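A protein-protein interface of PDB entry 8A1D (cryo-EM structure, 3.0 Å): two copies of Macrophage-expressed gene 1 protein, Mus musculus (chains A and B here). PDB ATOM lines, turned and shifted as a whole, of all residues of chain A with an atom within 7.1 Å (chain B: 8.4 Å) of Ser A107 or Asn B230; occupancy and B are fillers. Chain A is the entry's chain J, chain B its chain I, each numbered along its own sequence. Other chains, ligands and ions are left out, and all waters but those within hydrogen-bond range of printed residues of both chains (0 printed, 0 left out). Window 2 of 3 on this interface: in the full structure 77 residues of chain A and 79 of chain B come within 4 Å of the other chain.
N of Phe A106 sits at hydrogen-bond distance from O of Ile B231 (2.4 Å).
The backbone carbonyl oxygen of Asn B233 sits at hydrogen-bond distance from the backbone NH of Ala A104, at 2.6 Å.
O of Ala A104 touches O of Ile B231 (3.8 Å).
Ala A104 touches Val B232 (O to CA, 3.3 Å).
O of Ile B231 touches C of Leu A105, at 3.4 Å.
CD2 of Leu A105 touches CG2 of Val B232 (3.96 Å).
Asn B230 touches Ser A107 (O to CB, 3.8 Å).
Ile B231 touches Ser A107.
Of the printed residues of chain B, Ala A104 touches Ile B231 (3.8 Å), Val B232 (3.3 Å) and Asn B233 (2.6 Å).
Of the printed residues of chain B, Leu A105 touches Ile B231 (3.4 Å) and Val B232 (3.96 Å).
Printed residues of chain B within 4 Å of Phe A106: Ile B231 (2.4 Å).
Printed residues of chain B within 4 Å of Ser A107: Asn B230 (3.8 Å) and Ile B231 (3.98 Å).
Asn B230 touches just one residue of chain A: Ser A107.
The nearest residue of chain A that does not touch Asn B230 is Phe A106 (4.3 Å).
Of the 8 printed residues of chain A, 4 touch a printed residue of chain B.
Hydrophobic or aromatic side chains of chain A that line the printed part of chain B: Ala A104 and Leu A105.
Of the 8 printed residues of chain B, 4 touch a printed residue of chain A.
2 positions are printed for both chains.
Of the 8 pairs that touch across the chains among the printed residues, none has its exchanged pair printed and touching as well.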
ATOM      1  N   ALA A 104      10.611 -13.591 -16.493  1.00  0.00           N
ATOM      2  CA  ALA A 104      10.624 -12.155 -16.244  1.00  0.00           C
ATOM      3  C   ALA A 104      12.025 -11.629 -16.509  1.00  0.00           C
ATOM      4  O   ALA A 104      12.986 -12.059 -15.865  1.00  0.00           O
ATOM      5  CB  ALA A 104      10.186 -11.838 -14.813  1.00  0.00           C
ATOM      6  N   LEU A 105      12.136 -10.702 -17.453  1.00  0.00           N
ATOM      7  CA  LEU A 105      13.399 -10.076 -17.816  1.00  0.00           C
ATOM      8  C   LEU A 105      13.381  -8.634 -17.340  1.00  0.00           C
ATOM      9  O   LEU A 105      12.406  -7.909 -17.576  1.00  0.00           O
ATOM     10  CB  LEU A 105      13.641 -10.134 -19.326  1.00  0.00           C
ATOM     11  CG  LEU A 105      13.888 -11.495 -19.972  1.00  0.00           C
ATOM     12  CD1 LEU A 105      14.129 -11.340 -21.461  1.00  0.00           C
ATOM     13  CD2 LEU A 105      15.073 -12.167 -19.322  1.00  0.00           C
ATOM     14  N   PHE A 106      14.448  -8.234 -16.652  1.00  0.00           N
ATOM     15  CA  PHE A 106      14.699  -6.857 -16.242  1.00  0.00           C
ATOM     16  C   PHE A 106      13.595  -6.303 -15.356  1.00  0.00           C
ATOM     17  O   PHE A 106      13.446  -5.085 -15.239  1.00  0.00           O
ATOM     18  CB  PHE A 106      14.900  -5.954 -17.460  1.00  0.00           C
ATOM     19  CG  PHE A 106      15.908  -6.479 -18.431  1.00  0.00           C
ATOM     20  CD1 PHE A 106      17.256  -6.252 -18.245  1.00  0.00           C
ATOM     21  CD2 PHE A 106      15.503  -7.197 -19.540  1.00  0.00           C
ATOM     22  CE1 PHE A 106      18.183  -6.742 -19.142  1.00  0.00           C
ATOM     23  CE2 PHE A 106      16.423  -7.685 -20.441  1.00  0.00           C
ATOM     24  CZ  PHE A 106      17.764  -7.458 -20.242  1.00  0.00           C
ATOM     25  N   SER A 107      12.816  -7.184 -14.728  1.00  0.00           N
ATOM     26  CA  SER A 107      11.671  -6.804 -13.906  1.00  0.00           C
ATOM     27  C   SER A 107      10.650  -5.977 -14.681  1.00  0.00           C
ATOM     28  O   SER A 107       9.866  -5.234 -14.083  1.00  0.00           O
ATOM     29  CB  SER A 107      12.112  -6.052 -12.646  1.00  0.00           C
ATOM     30  OG  SER A 107      10.993  -5.678 -11.866  1.00  0.00           O
ATOM     31  N   ARG A 108      10.653  -6.077 -16.001  1.00  0.00           N
ATOM     32  CA  ARG A 108       9.688  -5.361 -16.827  1.00  0.00           C
ATOM     33  C   ARG A 108       8.975  -6.255 -17.827  1.00  0.00           C
ATOM     34  O   ARG A 108       7.766  -6.110 -18.014  1.00  0.00           O
ATOM     35  CB  ARG A 108      10.385  -4.214 -17.572  1.00  0.00           C
ATOM     36  CG  ARG A 108      11.027  -3.182 -16.669  1.00  0.00           C
ATOM     37  CD  ARG A 108      11.611  -2.041 -17.483  1.00  0.00           C
ATOM     38  NE  ARG A 108      12.532  -2.527 -18.504  1.00  0.00           N
ATOM     39  CZ  ARG A 108      13.214  -1.746 -19.331  1.00  0.00           C
ATOM     40  NH1 ARG A 108      13.118  -0.429 -19.274  1.00  0.00           N
ATOM     41  NH2 ARG A 108      14.013  -2.303 -20.237  1.00  0.00           N
ATOM     42  N   VAL A 109       9.682  -7.184 -18.462  1.00  0.00           N
ATOM     43  CA  VAL A 109       9.121  -8.009 -19.526  1.00  0.00           C
ATOM     44  C   VAL A 109       8.692  -9.327 -18.896  1.00  0.00           C
ATOM     45  O   VAL A 109       9.527 -10.113 -18.453  1.00  0.00           O
ATOM     46  CB  VAL A 109      10.122  -8.223 -20.662  1.00  0.00           C
ATOM     47  CG1 VAL A 109       9.527  -9.109 -21.735  1.00  0.00           C
ATOM     48  CG2 VAL A 109      10.550  -6.892 -21.245  1.00  0.00           C
ATOM     49  N   ASN A 110       7.389  -9.581 -18.856  1.00  0.00           N
ATOM     50  CA  ASN A 110       6.838 -10.785 -18.254  1.00  0.00           C
ATOM     51  C   ASN A 110       6.306 -11.711 -19.335  1.00  0.00           C
ATOM     52  O   ASN A 110       5.845 -11.254 -20.382  1.00  0.00           O
ATOM     53  CB  ASN A 110       5.714 -10.446 -17.275  1.00  0.00           C
ATOM     54  CG  ASN A 110       6.163  -9.515 -16.178  1.00  0.00           C
ATOM     55  OD1 ASN A 110       7.152  -8.800 -16.322  1.00  0.00           O
ATOM     56  ND2 ASN A 110       5.439  -9.519 -15.066  1.00  0.00           N
ATOM     57  N   ALA A 227       6.225  -3.791 -19.546  1.00  0.00           N
ATOM     58  CA  ALA A 227       5.843  -2.686 -18.678  1.00  0.00           C
ATOM     59  C   ALA A 227       7.051  -1.794 -18.437  1.00  0.00           C
ATOM     60  O   ALA A 227       7.885  -2.095 -17.578  1.00  0.00           O
ATOM     61  CB  ALA A 227       5.279  -3.201 -17.353  1.00  0.00           C
ATOM     62  N   ARG B 108      19.679 -19.277  -5.331  1.00  0.00           N
ATOM     63  CA  ARG B 108      18.936 -18.731  -6.459  1.00  0.00           C
ATOM     64  C   ARG B 108      18.370 -19.805  -7.372  1.00  0.00           C
ATOM     65  O   ARG B 108      17.220 -19.693  -7.797  1.00  0.00           O
ATOM     66  CB  ARG B 108      19.827 -17.793  -7.279  1.00  0.00           C
ATOM     67  CG  ARG B 108      20.396 -16.630  -6.503  1.00  0.00           C
ATOM     68  CD  ARG B 108      21.210 -15.739  -7.418  1.00  0.00           C
ATOM     69  NE  ARG B 108      22.204 -16.503  -8.163  1.00  0.00           N
ATOM     70  CZ  ARG B 108      23.096 -15.970  -8.986  1.00  0.00           C
ATOM     71  NH1 ARG B 108      23.169 -14.663  -9.172  1.00  0.00           N
ATOM     72  NH2 ARG B 108      23.937 -16.769  -9.637  1.00  0.00           N
ATOM     73  N   ALA B 227      16.262 -17.593 -10.294  1.00  0.00           N
ATOM     74  CA  ALA B 227      15.847 -16.268  -9.846  1.00  0.00           C
ATOM     75  C   ALA B 227      17.081 -15.453  -9.485  1.00  0.00           C
ATOM     76  O   ALA B 227      17.638 -15.614  -8.393  1.00  0.00           O
ATOM     77  CB  ALA B 227      14.890 -16.369  -8.661  1.00  0.00           C
ATOM     78  N   PHE B 228      17.493 -14.569 -10.391  1.00  0.00           N
ATOM     79  CA  PHE B 228      18.576 -13.629 -10.126  1.00  0.00           C
ATOM     80  C   PHE B 228      18.085 -12.529  -9.189  1.00  0.00           C
ATOM     81  O   PHE B 228      17.008 -12.610  -8.593  1.00  0.00           O
ATOM     82  CB  PHE B 228      19.109 -13.036 -11.426  1.00  0.00           C
ATOM     83  CG  PHE B 228      20.107 -13.897 -12.140  1.00  0.00           C
ATOM     84  CD1 PHE B 228      21.457 -13.777 -11.866  1.00  0.00           C
ATOM     85  CD2 PHE B 228      19.705 -14.808 -13.097  1.00  0.00           C
ATOM     86  CE1 PHE B 228      22.384 -14.556 -12.528  1.00  0.00           C
ATOM     87  CE2 PHE B 228      20.630 -15.591 -13.762  1.00  0.00           C
ATOM     88  CZ  PHE B 228      21.969 -15.465 -13.476  1.00  0.00           C
ATOM     89  N   LEU B 229      18.889 -11.476  -9.048  1.00  0.00           N
ATOM     90  CA  LEU B 229      18.549 -10.340  -8.194  1.00  0.00           C
ATOM     91  C   LEU B 229      17.736  -9.321  -8.994  1.00  0.00           C
ATOM     92  O   LEU B 229      18.214  -8.254  -9.384  1.00  0.00           O
ATOM     93  CB  LEU B 229      19.808  -9.716  -7.611  1.00  0.00           C
ATOM     94  CG  LEU B 229      20.403 -10.366  -6.358  1.00  0.00           C
ATOM     95  CD1 LEU B 229      21.151 -11.655  -6.692  1.00  0.00           C
ATOM     96  CD2 LEU B 229      21.314  -9.387  -5.634  1.00  0.00           C
ATOM     97  N   ASN B 230      16.479  -9.682  -9.247  1.00  0.00           N
ATOM     98  CA  ASN B 230      15.501  -8.780  -9.853  1.00  0.00           C
ATOM     99  C   ASN B 230      15.943  -8.290 -11.228  1.00  0.00           C
ATOM    100  O   ASN B 230      15.629  -7.169 -11.630  1.00  0.00           O
ATOM    101  CB  ASN B 230      15.206  -7.596  -8.932  1.00  0.00           C
ATOM    102  CG  ASN B 230      14.757  -8.037  -7.558  1.00  0.00           C
ATOM    103  OD1 ASN B 230      15.010  -9.169  -7.146  1.00  0.00           O
ATOM    104  ND2 ASN B 230      14.077  -7.150  -6.843  1.00  0.00           N
ATOM    105  N   ILE B 231      16.691  -9.120 -11.949  1.00  0.00           N
ATOM    106  CA  ILE B 231      17.036  -8.875 -13.343  1.00  0.00           C
ATOM    107  C   ILE B 231      16.450  -9.943 -14.257  1.00  0.00           C
ATOM    108  O   ILE B 231      15.897  -9.636 -15.317  1.00  0.00           O
ATOM    109  CB  ILE B 231      18.564  -8.765 -13.537  1.00  0.00           C
ATOM    110  CG1 ILE B 231      18.923  -8.916 -15.016  1.00  0.00           C
ATOM    111  CG2 ILE B 231      19.294  -9.772 -12.674  1.00  0.00           C
ATOM    112  CD1 ILE B 231      20.382  -8.713 -15.312  1.00  0.00           C
ATOM    113  N   VAL B 232      16.556 -11.208 -13.861  1.00  0.00           N
ATOM    114  CA  VAL B 232      16.037 -12.323 -14.642  1.00  0.00           C
ATOM    115  C   VAL B 232      15.297 -13.261 -13.702  1.00  0.00           C
ATOM    116  O   VAL B 232      15.791 -13.572 -12.613  1.00  0.00           O
ATOM    117  CB  VAL B 232      17.159 -13.071 -15.388  1.00  0.00           C
ATOM    118  CG1 VAL B 232      16.628 -14.345 -16.013  1.00  0.00           C
ATOM    119  CG2 VAL B 232      17.790 -12.177 -16.443  1.00  0.00           C
ATOM    120  N   ASN B 233      14.106 -13.687 -14.109  1.00  0.00           N
ATOM    121  CA  ASN B 233      13.351 -14.715 -13.401  1.00  0.00           C
ATOM    122  C   ASN B 233      12.843 -15.707 -14.432  1.00  0.00           C
ATOM    123  O   ASN B 233      12.265 -15.303 -15.442  1.00  0.00           O
ATOM    124  CB  ASN B 233      12.190 -14.108 -12.611  1.00  0.00           C
ATOM    125  CG  ASN B 233      11.595 -15.079 -11.621  1.00  0.00           C
ATOM    126  OD1 ASN B 233      11.590 -16.288 -11.844  1.00  0.00           O
ATOM    127  ND2 ASN B 233      11.096 -14.554 -10.511  1.00  0.00           N
